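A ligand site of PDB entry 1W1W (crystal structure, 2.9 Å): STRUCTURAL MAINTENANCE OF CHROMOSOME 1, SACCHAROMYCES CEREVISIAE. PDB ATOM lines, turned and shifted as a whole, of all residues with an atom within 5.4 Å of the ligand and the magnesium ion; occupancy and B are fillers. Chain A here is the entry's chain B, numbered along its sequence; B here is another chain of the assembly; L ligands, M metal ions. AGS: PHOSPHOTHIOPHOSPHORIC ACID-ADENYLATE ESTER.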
ATOM      1  N   PHE A  12      23.277  13.270   5.356  1.00  0.00           N
ATOM      2  CA  PHE A  12      23.735  14.652   5.363  1.00  0.00           C
ATOM      3  C   PHE A  12      25.092  14.908   5.970  1.00  0.00           C
ATOM      4  O   PHE A  12      26.012  15.335   5.267  1.00  0.00           O
ATOM      5  CB  PHE A  12      22.736  15.622   5.976  1.00  0.00           C
ATOM      6  CG  PHE A  12      23.139  17.064   5.772  1.00  0.00           C
ATOM      7  CD1 PHE A  12      23.486  17.863   6.853  1.00  0.00           C
ATOM      8  CD2 PHE A  12      23.298  17.558   4.487  1.00  0.00           C
ATOM      9  CE1 PHE A  12      23.996  19.148   6.640  1.00  0.00           C
ATOM     10  CE2 PHE A  12      23.807  18.829   4.275  1.00  0.00           C
ATOM     11  CZ  PHE A  12      24.159  19.620   5.347  1.00  0.00           C
ATOM     12  N   LYS A  13      25.260  14.719   7.268  1.00  0.00           N
ATOM     13  CA  LYS A  13      26.600  14.925   7.769  1.00  0.00           C
ATOM     14  C   LYS A  13      26.890  13.804   8.734  1.00  0.00           C
ATOM     15  O   LYS A  13      27.622  12.879   8.418  1.00  0.00           O
ATOM     16  CB  LYS A  13      26.769  16.296   8.452  1.00  0.00           C
ATOM     17  CG  LYS A  13      26.743  17.470   7.476  1.00  0.00           C
ATOM     18  CD  LYS A  13      27.132  18.797   8.119  1.00  0.00           C
ATOM     19  CE  LYS A  13      28.605  18.827   8.519  1.00  0.00           C
ATOM     20  NZ  LYS A  13      29.022  20.151   9.089  1.00  0.00           N
ATOM     21  N   SER A  14      26.284  13.875   9.900  1.00  0.00           N
ATOM     22  CA  SER A  14      26.470  12.864  10.907  1.00  0.00           C
ATOM     23  C   SER A  14      25.155  12.107  10.910  1.00  0.00           C
ATOM     24  O   SER A  14      24.973  11.177  11.697  1.00  0.00           O
ATOM     25  CB  SER A  14      26.709  13.528  12.252  1.00  0.00           C
ATOM     26  OG  SER A  14      25.615  14.361  12.573  1.00  0.00           O
ATOM     27  N   GLY A  33      20.621  18.558  23.036  1.00  0.00           N
ATOM     28  CA  GLY A  33      21.354  17.317  23.016  1.00  0.00           C
ATOM     29  C   GLY A  33      22.751  17.579  23.507  1.00  0.00           C
ATOM     30  O   GLY A  33      23.162  18.735  23.557  1.00  0.00           O
ATOM     31  N   PRO A  34      23.504  16.542  23.883  1.00  0.00           N
ATOM     32  CA  PRO A  34      24.875  16.708  24.375  1.00  0.00           C
ATOM     33  C   PRO A  34      25.867  17.179  23.308  1.00  0.00           C
ATOM     34  O   PRO A  34      25.600  17.138  22.109  1.00  0.00           O
ATOM     35  CB  PRO A  34      25.232  15.325  24.899  1.00  0.00           C
ATOM     36  CG  PRO A  34      24.451  14.415  23.992  1.00  0.00           C
ATOM     37  CD  PRO A  34      23.108  15.118  23.975  1.00  0.00           C
ATOM     38  N   ASN A  35      27.023  17.633  23.789  1.00  0.00           N
ATOM     39  CA  ASN A  35      28.105  18.097  22.925  1.00  0.00           C
ATOM     40  C   ASN A  35      28.456  17.005  21.905  1.00  0.00           C
ATOM     41  O   ASN A  35      28.513  15.819  22.234  1.00  0.00           O
ATOM     42  CB  ASN A  35      29.344  18.439  23.769  1.00  0.00           C
ATOM     43  CG  ASN A  35      29.269  19.836  24.415  1.00  0.00           C
ATOM     44  OD1 ASN A  35      30.053  20.165  25.306  1.00  0.00           O
ATOM     45  ND2 ASN A  35      28.335  20.644  23.954  1.00  0.00           N
ATOM     46  N   GLY A  36      28.688  17.416  20.670  1.00  0.00           N
ATOM     47  CA  GLY A  36      29.050  16.472  19.637  1.00  0.00           C
ATOM     48  C   GLY A  36      27.923  15.622  19.093  1.00  0.00           C
ATOM     49  O   GLY A  36      28.167  14.838  18.181  1.00  0.00           O
ATOM     50  N   SER A  37      26.701  15.772  19.601  1.00  0.00           N
ATOM     51  CA  SER A  37      25.610  14.924  19.134  1.00  0.00           C
ATOM     52  C   SER A  37      25.153  15.230  17.715  1.00  0.00           C
ATOM     53  O   SER A  37      24.625  14.353  17.031  1.00  0.00           O
ATOM     54  CB  SER A  37      24.421  14.934  20.113  1.00  0.00           C
ATOM     55  OG  SER A  37      23.662  16.130  20.068  1.00  0.00           O
ATOM     56  N   GLY A  38      25.346  16.459  17.247  1.00  0.00           N
ATOM     57  CA  GLY A  38      24.953  16.778  15.891  1.00  0.00           C
ATOM     58  C   GLY A  38      23.891  17.840  15.707  1.00  0.00           C
ATOM     59  O   GLY A  38      23.169  17.850  14.701  1.00  0.00           O
ATOM     60  N   LYS A  39      23.798  18.753  16.674  1.00  0.00           N
ATOM     61  CA  LYS A  39      22.797  19.811  16.604  1.00  0.00           C
ATOM     62  C   LYS A  39      23.125  20.855  15.531  1.00  0.00           C
ATOM     63  O   LYS A  39      22.261  21.223  14.735  1.00  0.00           O
ATOM     64  CB  LYS A  39      22.675  20.486  17.976  1.00  0.00           C
ATOM     65  CG  LYS A  39      22.203  19.508  19.028  1.00  0.00           C
ATOM     66  CD  LYS A  39      21.911  20.177  20.347  1.00  0.00           C
ATOM     67  CE  LYS A  39      23.173  20.752  20.959  1.00  0.00           C
ATOM     68  NZ  LYS A  39      24.319  19.807  21.045  1.00  0.00           N
ATOM     69  N   SER A  40      24.369  21.304  15.509  1.00  0.00           N
ATOM     70  CA  SER A  40      24.750  22.299  14.525  1.00  0.00           C
ATOM     71  C   SER A  40      24.693  21.701  13.126  1.00  0.00           C
ATOM     72  O   SER A  40      24.374  22.419  12.175  1.00  0.00           O
ATOM     73  CB  SER A  40      26.137  22.833  14.845  1.00  0.00           C
ATOM     74  OG  SER A  40      26.105  23.629  16.017  1.00  0.00           O
ATOM     75  N   ASN A  41      24.963  20.404  12.977  1.00  0.00           N
ATOM     76  CA  ASN A  41      24.893  19.757  11.663  1.00  0.00           C
ATOM     77  C   ASN A  41      23.459  19.909  11.194  1.00  0.00           C
ATOM     78  O   ASN A  41      23.207  20.084  10.017  1.00  0.00           O
ATOM     79  CB  ASN A  41      25.239  18.265  11.753  1.00  0.00           C
ATOM     80  CG  ASN A  41      26.727  18.016  11.932  1.00  0.00           C
ATOM     81  OD1 ASN A  41      27.546  18.693  11.331  1.00  0.00           O
ATOM     82  ND2 ASN A  41      27.076  17.018  12.750  1.00  0.00           N
ATOM     83  N   MET A  42      22.525  19.877  12.130  1.00  0.00           N
ATOM     84  CA  MET A  42      21.105  20.027  11.821  1.00  0.00           C
ATOM     85  C   MET A  42      20.791  21.419  11.291  1.00  0.00           C
ATOM     86  O   MET A  42      19.842  21.607  10.528  1.00  0.00           O
ATOM     87  CB  MET A  42      20.292  19.759  13.075  1.00  0.00           C
ATOM     88  CG  MET A  42      19.391  18.564  12.968  1.00  0.00           C
ATOM     89  SD  MET A  42      17.984  18.966  11.983  1.00  0.00           S
ATOM     90  CE  MET A  42      16.993  19.751  13.254  1.00  0.00           C
ATOM     91  N   ASP A  64      32.206  17.656   1.605  1.00  0.00           N
ATOM     92  CA  ASP A  64      32.496  17.434   3.024  1.00  0.00           C
ATOM     93  C   ASP A  64      31.226  17.369   3.855  1.00  0.00           C
ATOM     94  O   ASP A  64      31.278  17.216   5.082  1.00  0.00           O
ATOM     95  CB  ASP A  64      33.432  18.515   3.579  1.00  0.00           C
ATOM     96  CG  ASP A  64      34.890  18.295   3.164  1.00  0.00           C
ATOM     97  OD1 ASP A  64      35.788  18.802   3.879  1.00  0.00           O
ATOM     98  OD2 ASP A  64      35.128  17.609   2.134  1.00  0.00           O
ATOM     99  N   LEU A  65      30.083  17.533   3.194  1.00  0.00           N
ATOM    100  CA  LEU A  65      28.801  17.395   3.841  1.00  0.00           C
ATOM    101  C   LEU A  65      28.663  15.869   3.702  1.00  0.00           C
ATOM    102  O   LEU A  65      29.354  15.163   4.411  1.00  0.00           O
ATOM    103  CB  LEU A  65      27.745  18.197   3.081  1.00  0.00           C
ATOM    104  CG  LEU A  65      28.149  19.690   2.964  1.00  0.00           C
ATOM    105  CD1 LEU A  65      27.107  20.452   2.175  1.00  0.00           C
ATOM    106  CD2 LEU A  65      28.313  20.308   4.331  1.00  0.00           C
ATOM    107  N   ILE A  66      27.851  15.341   2.788  1.00  0.00           N
ATOM    108  CA  ILE A  66      27.772  13.872   2.578  1.00  0.00           C
ATOM    109  C   ILE A  66      28.375  12.971   3.695  1.00  0.00           C
ATOM    110  O   ILE A  66      29.594  12.943   3.904  1.00  0.00           O
ATOM    111  CB  ILE A  66      28.514  13.452   1.284  1.00  0.00           C
ATOM    112  CG1 ILE A  66      28.071  14.314   0.103  1.00  0.00           C
ATOM    113  CG2 ILE A  66      28.269  11.970   1.011  1.00  0.00           C
ATOM    114  CD1 ILE A  66      26.967  13.723  -0.706  1.00  0.00           C
ATOM    115  N   TYR A  67      27.520  12.190   4.358  1.00  0.00           N
ATOM    116  CA  TYR A  67      27.956  11.297   5.431  1.00  0.00           C
ATOM    117  C   TYR A  67      29.232  10.517   5.138  1.00  0.00           C
ATOM    118  O   TYR A  67      29.560  10.230   3.987  1.00  0.00           O
ATOM    119  CB  TYR A  67      26.842  10.303   5.764  1.00  0.00           C
ATOM    120  CG  TYR A  67      27.235   9.301   6.830  1.00  0.00           C
ATOM    121  CD1 TYR A  67      27.234   9.638   8.195  1.00  0.00           C
ATOM    122  CD2 TYR A  67      27.616   8.001   6.488  1.00  0.00           C
ATOM    123  CE1 TYR A  67      27.605   8.709   9.167  1.00  0.00           C
ATOM    124  CE2 TYR A  67      27.980   7.065   7.461  1.00  0.00           C
ATOM    125  CZ  TYR A  67      27.965   7.431   8.796  1.00  0.00           C
ATOM    126  OH  TYR A  67      28.289   6.489   9.733  1.00  0.00           O
ATOM    127  N   ARG A  68      29.944  10.156   6.212  1.00  0.00           N
ATOM    128  CA  ARG A  68      31.206   9.402   6.120  1.00  0.00           C
ATOM    129  C   ARG A  68      31.313   8.330   7.221  1.00  0.00           C
ATOM    130  O   ARG A  68      31.344   8.655   8.412  1.00  0.00           O
ATOM    131  CB  ARG A  68      32.398  10.343   6.247  1.00  0.00           C
ATOM    132  CG  ARG A  68      32.686  11.140   5.006  1.00  0.00           C
ATOM    133  CD  ARG A  68      33.736  10.451   4.165  1.00  0.00           C
ATOM    134  NE  ARG A  68      34.760  11.389   3.714  1.00  0.00           N
ATOM    135  CZ  ARG A  68      35.455  12.206   4.506  1.00  0.00           C
ATOM    136  NH1 ARG A  68      36.377  13.013   3.986  1.00  0.00           N
ATOM    137  NH2 ARG A  68      35.225  12.252   5.817  1.00  0.00           N
ATOM    138  N   GLN A 151      26.680  29.045  15.234  1.00  0.00           N
ATOM    139  CA  GLN A 151      27.411  28.864  16.494  1.00  0.00           C
ATOM    140  C   GLN A 151      28.668  29.728  16.579  1.00  0.00           C
ATOM    141  O   GLN A 151      29.530  29.716  15.695  1.00  0.00           O
ATOM    142  CB  GLN A 151      27.745  27.375  16.686  1.00  0.00           C
ATOM    143  CG  GLN A 151      28.750  27.039  17.788  1.00  0.00           C
ATOM    144  CD  GLN A 151      28.396  25.761  18.529  1.00  0.00           C
ATOM    145  OE1 GLN A 151      27.722  24.870  17.982  1.00  0.00           O
ATOM    146  NE2 GLN A 151      28.855  25.646  19.771  1.00  0.00           N
ATOM    147  N   ASP A 362      21.854  29.278  16.762  1.00  0.00           N
ATOM    148  CA  ASP A 362      22.641  28.216  17.378  1.00  0.00           C
ATOM    149  C   ASP A 362      22.839  28.582  18.842  1.00  0.00           C
ATOM    150  O   ASP A 362      21.880  28.924  19.529  1.00  0.00           O
ATOM    151  CB  ASP A 362      23.985  27.997  16.662  1.00  0.00           C
ATOM    152  CG  ASP A 362      24.448  26.520  16.679  1.00  0.00           C
ATOM    153  OD1 ASP A 362      25.094  26.061  15.710  1.00  0.00           O
ATOM    154  OD2 ASP A 362      24.177  25.812  17.669  1.00  0.00           O
ATOM    155  N   GLU A 363      24.052  28.561  19.364  1.00  0.00           N
ATOM    156  CA  GLU A 363      24.171  28.840  20.792  1.00  0.00           C
ATOM    157  C   GLU A 363      24.208  30.313  21.158  1.00  0.00           C
ATOM    158  O   GLU A 363      25.116  30.752  21.847  1.00  0.00           O
ATOM    159  CB  GLU A 363      25.391  28.128  21.347  1.00  0.00           C
ATOM    160  CG  GLU A 363      25.380  26.651  21.049  1.00  0.00           C
ATOM    161  CD  GLU A 363      25.131  25.820  22.289  1.00  0.00           C
ATOM    162  OE1 GLU A 363      24.045  25.950  22.905  1.00  0.00           O
ATOM    163  OE2 GLU A 363      26.043  25.034  22.639  1.00  0.00           O
ATOM    164  N   LEU A 395      22.044  24.678  25.086  1.00  0.00           N
ATOM    165  CA  LEU A 395      22.447  23.633  26.013  1.00  0.00           C
ATOM    166  C   LEU A 395      21.808  23.919  27.377  1.00  0.00           C
ATOM    167  O   LEU A 395      21.816  23.061  28.260  1.00  0.00           O
ATOM    168  CB  LEU A 395      23.957  23.618  26.191  1.00  0.00           C
ATOM    169  CG  LEU A 395      24.809  23.181  25.018  1.00  0.00           C
ATOM    170  CD1 LEU A 395      26.279  23.412  25.342  1.00  0.00           C
ATOM    171  CD2 LEU A 395      24.537  21.716  24.746  1.00  0.00           C
ATOM    172  N   ARG A 411      23.605  10.574  19.840  1.00  0.00           N
ATOM    173  CA  ARG A 411      24.449   9.725  19.002  1.00  0.00           C
ATOM    174  C   ARG A 411      24.092   8.268  19.263  1.00  0.00           C
ATOM    175  O   ARG A 411      23.522   7.923  20.307  1.00  0.00           O
ATOM    176  CB  ARG A 411      25.931   9.953  19.306  1.00  0.00           C
ATOM    177  CG  ARG A 411      26.529  11.205  18.683  1.00  0.00           C
ATOM    178  CD  ARG A 411      26.487  11.151  17.159  1.00  0.00           C
ATOM    179  NE  ARG A 411      27.737  10.769  16.495  1.00  0.00           N
ATOM    180  CZ  ARG A 411      28.543   9.761  16.863  1.00  0.00           C
ATOM    181  NH1 ARG A 411      29.644   9.530  16.163  1.00  0.00           N
ATOM    182  NH2 ARG A 411      28.275   9.018  17.937  1.00  0.00           N
ATOM    183  N   ASN A 416      27.234   4.770  14.401  1.00  0.00           N
ATOM    184  CA  ASN A 416      27.975   6.006  14.108  1.00  0.00           C
ATOM    185  C   ASN A 416      27.124   7.018  13.331  1.00  0.00           C
ATOM    186  O   ASN A 416      27.437   7.379  12.201  1.00  0.00           O
ATOM    187  CB  ASN A 416      29.252   5.709  13.314  1.00  0.00           C
ATOM    188  CG  ASN A 416      30.028   6.986  12.963  1.00  0.00           C
ATOM    189  OD1 ASN A 416      30.218   7.854  13.804  1.00  0.00           O
ATOM    190  ND2 ASN A 416      30.469   7.091  11.710  1.00  0.00           N
ATOM    191  N   PRO B 323      37.918  13.007  19.940  1.00  0.00           N
ATOM    192  CA  PRO B 323      37.094  12.755  21.123  1.00  0.00           C
ATOM    193  C   PRO B 323      36.816  11.272  21.197  1.00  0.00           C
ATOM    194  O   PRO B 323      36.850  10.591  20.187  1.00  0.00           O
ATOM    195  CB  PRO B 323      35.836  13.590  20.845  1.00  0.00           C
ATOM    196  CG  PRO B 323      35.767  13.615  19.368  1.00  0.00           C
ATOM    197  CD  PRO B 323      37.203  13.834  18.961  1.00  0.00           C
ATOM    198  N   LYS B 326      34.260   8.642  18.982  1.00  0.00           N
ATOM    199  CA  LYS B 326      34.290   9.062  17.575  1.00  0.00           C
ATOM    200  C   LYS B 326      35.598   8.637  16.909  1.00  0.00           C
ATOM    201  O   LYS B 326      36.355   7.830  17.458  1.00  0.00           O
ATOM    202  CB  LYS B 326      34.118  10.575  17.475  1.00  0.00           C
ATOM    203  CG  LYS B 326      32.857  11.075  18.162  1.00  0.00           C
ATOM    204  CD  LYS B 326      32.600  12.536  17.843  1.00  0.00           C
ATOM    205  CE  LYS B 326      31.349  13.043  18.547  1.00  0.00           C
ATOM    206  NZ  LYS B 326      30.167  12.200  18.241  1.00  0.00           N
ATOM    207  N   PHE B 328      38.011  10.864  14.138  1.00  0.00           N
ATOM    208  CA  PHE B 328      38.376  11.860  13.135  1.00  0.00           C
ATOM    209  C   PHE B 328      39.587  12.535  13.755  1.00  0.00           C
ATOM    210  O   PHE B 328      39.945  12.215  14.892  1.00  0.00           O
ATOM    211  CB  PHE B 328      37.233  12.859  12.934  1.00  0.00           C
ATOM    212  CG  PHE B 328      36.389  12.598  11.690  1.00  0.00           C
ATOM    213  CD1 PHE B 328      35.057  13.032  11.632  1.00  0.00           C
ATOM    214  CD2 PHE B 328      36.935  11.974  10.573  1.00  0.00           C
ATOM    215  CE1 PHE B 328      34.279  12.821  10.478  1.00  0.00           C
ATOM    216  CE2 PHE B 328      36.169  11.761   9.408  1.00  0.00           C
ATOM    217  CZ  PHE B 328      34.839  12.196   9.370  1.00  0.00           C
ATOM    218  N   TYR B 333      36.564  18.981  12.053  1.00  0.00           N
ATOM    219  CA  TYR B 333      35.404  18.128  12.309  1.00  0.00           C
ATOM    220  C   TYR B 333      34.877  18.170  13.742  1.00  0.00           C
ATOM    221  O   TYR B 333      33.739  17.765  13.991  1.00  0.00           O
ATOM    222  CB  TYR B 333      35.733  16.687  11.914  1.00  0.00           C
ATOM    223  CG  TYR B 333      35.972  16.496  10.432  1.00  0.00           C
ATOM    224  CD1 TYR B 333      37.097  17.069   9.807  1.00  0.00           C
ATOM    225  CD2 TYR B 333      35.075  15.775   9.642  1.00  0.00           C
ATOM    226  CE1 TYR B 333      37.307  16.920   8.426  1.00  0.00           C
ATOM    227  CE2 TYR B 333      35.272  15.628   8.272  1.00  0.00           C
ATOM    228  CZ  TYR B 333      36.392  16.197   7.669  1.00  0.00           C
ATOM    229  OH  TYR B 333      36.570  16.060   6.310  1.00  0.00           O
ATOM    230  N   LEU B 334      35.683  18.643  14.671  1.00  0.00           N
ATOM    231  CA  LEU B 334      35.258  18.740  16.048  1.00  0.00           C
ATOM    232  C   LEU B 334      34.148  19.789  16.202  1.00  0.00           C
ATOM    233  O   LEU B 334      34.066  20.728  15.411  1.00  0.00           O
ATOM    234  CB  LEU B 334      36.448  19.106  16.935  1.00  0.00           C
ATOM    235  CG  LEU B 334      37.541  18.055  17.056  1.00  0.00           C
ATOM    236  CD1 LEU B 334      38.615  18.534  18.007  1.00  0.00           C
ATOM    237  CD2 LEU B 334      36.933  16.758  17.552  1.00  0.00           C
ATOM    238  N   SER B 335      33.302  19.609  17.210  1.00  0.00           N
ATOM    239  CA  SER B 335      32.209  20.545  17.482  1.00  0.00           C
ATOM    240  C   SER B 335      32.697  21.645  18.435  1.00  0.00           C
ATOM    241  O   SER B 335      33.828  21.623  18.916  1.00  0.00           O
ATOM    242  CB  SER B 335      31.041  19.837  18.142  1.00  0.00           C
ATOM    243  OG  SER B 335      31.354  19.608  19.509  1.00  0.00           O
ATOM    244  N   GLY B 336      31.807  22.599  18.705  1.00  0.00           N
ATOM    245  CA  GLY B 336      32.159  23.681  19.603  1.00  0.00           C
ATOM    246  C   GLY B 336      32.717  23.136  20.889  1.00  0.00           C
ATOM    247  O   GLY B 336      33.851  23.448  21.262  1.00  0.00           O
ATOM    248  N   GLY B 337      31.934  22.297  21.559  1.00  0.00           N
ATOM    249  CA  GLY B 337      32.377  21.727  22.808  1.00  0.00           C
ATOM    250  C   GLY B 337      33.648  20.929  22.638  1.00  0.00           C
ATOM    251  O   GLY B 337      34.621  21.114  23.370  1.00  0.00           O
ATOM    252  N   GLU B 338      33.644  20.054  21.648  1.00  0.00           N
ATOM    253  CA  GLU B 338      34.797  19.229  21.412  1.00  0.00           C
ATOM    254  C   GLU B 338      36.058  20.046  21.218  1.00  0.00           C
ATOM    255  O   GLU B 338      37.087  19.756  21.830  1.00  0.00           O
ATOM    256  CB  GLU B 338      34.519  18.306  20.241  1.00  0.00           C
ATOM    257  CG  GLU B 338      33.581  17.183  20.647  1.00  0.00           C
ATOM    258  CD  GLU B 338      33.020  16.381  19.497  1.00  0.00           C
ATOM    259  OE1 GLU B 338      32.297  15.400  19.779  1.00  0.00           O
ATOM    260  OE2 GLU B 338      33.292  16.722  18.323  1.00  0.00           O
ATOM    261  N   ALA B 367      31.099  26.769  25.865  1.00  0.00           N
ATOM    262  CA  ALA B 367      30.538  25.853  24.875  1.00  0.00           C
ATOM    263  C   ALA B 367      30.323  24.430  25.381  1.00  0.00           C
ATOM    264  O   ALA B 367      29.843  23.576  24.629  1.00  0.00           O
ATOM    265  CB  ALA B 367      31.448  25.804  23.645  1.00  0.00           C
HETATM  266  PG  AGS L   1      28.199  21.384  20.240  1.00  0.00           P
HETATM  267  S1G AGS L   1      26.919  21.778  21.481  1.00  0.00           S
HETATM  268  O2G AGS L   1      29.515  21.012  20.809  1.00  0.00           O
HETATM  269  O3G AGS L   1      28.257  22.533  19.268  1.00  0.00           O
HETATM  270  PB  AGS L   1      26.827  19.776  18.258  1.00  0.00           P
HETATM  271  O1B AGS L   1      25.688  19.052  18.865  1.00  0.00           O
HETATM  272  O2B AGS L   1      26.497  21.041  17.579  1.00  0.00           O
HETATM  273  O3B AGS L   1      27.897  20.036  19.398  1.00  0.00           O
HETATM  274  PA  AGS L   1      27.640  19.085  15.647  1.00  0.00           P
HETATM  275  O1A AGS L   1      26.416  19.223  14.835  1.00  0.00           O
HETATM  276  O2A AGS L   1      28.674  20.155  15.729  1.00  0.00           O
HETATM  277  O3A AGS L   1      27.271  18.756  17.213  1.00  0.00           O
HETATM  278  O5' AGS L   1      28.241  17.652  15.313  1.00  0.00           O
HETATM  279  C5' AGS L   1      29.625  17.513  15.141  1.00  0.00           C
HETATM  280  C4' AGS L   1      29.920  16.020  15.075  1.00  0.00           C
HETATM  281  O4' AGS L   1      29.369  15.455  13.936  1.00  0.00           O
HETATM  282  C3' AGS L   1      31.410  15.671  15.100  1.00  0.00           C
HETATM  283  O3' AGS L   1      31.734  15.198  16.394  1.00  0.00           O
HETATM  284  C2' AGS L   1      31.563  14.551  14.062  1.00  0.00           C
HETATM  285  O2' AGS L   1      31.977  13.275  14.582  1.00  0.00           O
HETATM  286  C1' AGS L   1      30.194  14.502  13.350  1.00  0.00           C
HETATM  287  N9  AGS L   1      30.340  14.783  11.912  1.00  0.00           N
HETATM  288  C8  AGS L   1      30.610  15.945  11.199  1.00  0.00           C
HETATM  289  N7  AGS L   1      30.686  15.881   9.875  1.00  0.00           N
HETATM  290  C5  AGS L   1      30.459  14.539   9.680  1.00  0.00           C
HETATM  291  C6  AGS L   1      30.416  13.711   8.519  1.00  0.00           C
HETATM  292  N6  AGS L   1      30.586  14.265   7.198  1.00  0.00           N
HETATM  293  N1  AGS L   1      30.184  12.364   8.657  1.00  0.00           N
HETATM  294  C2  AGS L   1      29.978  11.808   9.911  1.00  0.00           C
HETATM  295  N3  AGS L   1      29.982  12.479  11.099  1.00  0.00           N
HETATM  296  C4  AGS L   1      30.249  13.840  10.926  1.00  0.00           C
HETATM  297 MG    MG M   1      27.650  22.940  17.494  1.00  0.00          MG
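Of the 34 residues printed, 2 come within 4 Å of the magnesium ion. The nearest printed residue that does not touch the magnesium ion is Gly 336 of chain B (4.3 Å).
N of Ser 40 lies within hydrogen-bond range of O1A of the ligand (3.0 Å). O of Lys 13 lies close to N6 of the ligand, 3.5 Å away. O1A of the ligand is in hydrogen-bond range of N of Asn 41, at 2.6 Å. An oxygen (O5') of the ligand lies within hydrogen-bond range of the side-chain amide nitrogen of Asn 41 (2.9 Å). The side-chain hydroxyl of Ser 335 of chain B is in hydrogen-bond range of an oxygen (O2G) of the ligand (2.7 Å). The backbone NH of Lys 39 lies within hydrogen-bond range of an oxygen (O1B) of the ligand (2.9 Å). An oxygen (O1B) of the ligand is in salt-bridge range of the side-chain amino group (NZ) of Lys 39 (2.7 Å). N of Gly 337 of chain B lies within hydrogen-bond range of O2G of the ligand. OE2 of Glu 338 of chain B sits at hydrogen-bond distance from O3' of the ligand, at 2.9 Å. An oxygen (O3A) of the ligand lies within hydrogen-bond range of the backbone NH (N) of Gly 38 (3.0 Å). The backbone NH of Gly 36 lies within hydrogen-bond range of an oxygen (O3B) of the ligand (3.0 Å). ND2 of Asn 35 sits close to S1G of the ligand (3.1 Å). A nitrogen (N6) of the ligand sits at hydrogen-bond distance from the backbone carbonyl oxygen of Leu 65, at 3.2 Å. The backbone NH of Arg 68 is in hydrogen-bond range of a nitrogen (N1) of the ligand (3.3 Å). N of Gly 336 of chain B is in hydrogen-bond range of O2G of the ligand (3.5 Å).
OE2 of Glu 363 sits close to S1G of the ligand (3.6 Å). CA of Ser 14 touches N3 of the ligand, at 3.5 Å. O of Pro 34 touches O1B of the ligand, at 3.8 Å. Ser 37 touches the ligand. Asp 64 touches the ligand. Ile 66 touches the ligand (O to N6, 3.7 Å). Tyr 67 touches the ligand (CD1 to C2, 3.9 Å). CE of Lys 326 of chain B touches O3' of the ligand (3.1 Å). O of Tyr 333 of chain B touches C3' of the ligand, at 3.3 Å. Hydrophobic or aromatic side chains within 4 Å of the ligand: Tyr 67.
The magnesium ion is bound by an oxygen (O3G) of the ligand (1.9 Å), the side-chain amide oxygen (OE1) of Gln 151 (2.0 Å), an oxygen (O2B) of the ligand (2.2 Å) and the side-chain hydroxyl (OG) of Ser 40 (2.2 Å).
The side-chain carboxylate (OD1) of Asp 362 lies close to the side-chain hydroxyl (OG) of Ser 40 (2.7 Å). The side-chain amino group (NZ) of Lys 13 lies close to the side-chain amide oxygen (OD1) of Asn 41, at 3.1 Å. The backbone carbonyl oxygen (O) of Gly 33 sits at hydrogen-bond distance from the side-chain amino group (NZ) of Lys 39, at 3.0 Å. The backbone carbonyl oxygen (O) of Ala 367 of chain B is in hydrogen-bond range of the side-chain amide nitrogen (ND2) of Asn 35, at 3.4 Å. The side-chain hydroxyl (OG) of Ser 37 sits at hydrogen-bond distance from the backbone carbonyl oxygen (O) of Pro 34, 3.0 Å away. OE1 of Glu 363 sits at hydrogen-bond distance from N of Leu 395. O of Phe 12 is in hydrogen-bond range of N of Ile 66 (3.1 Å). The backbone carbonyl oxygen (O) of Asn 416 sits at hydrogen-bond distance from the side-chain hydroxyl (OH) of Tyr 67 (2.8 Å).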
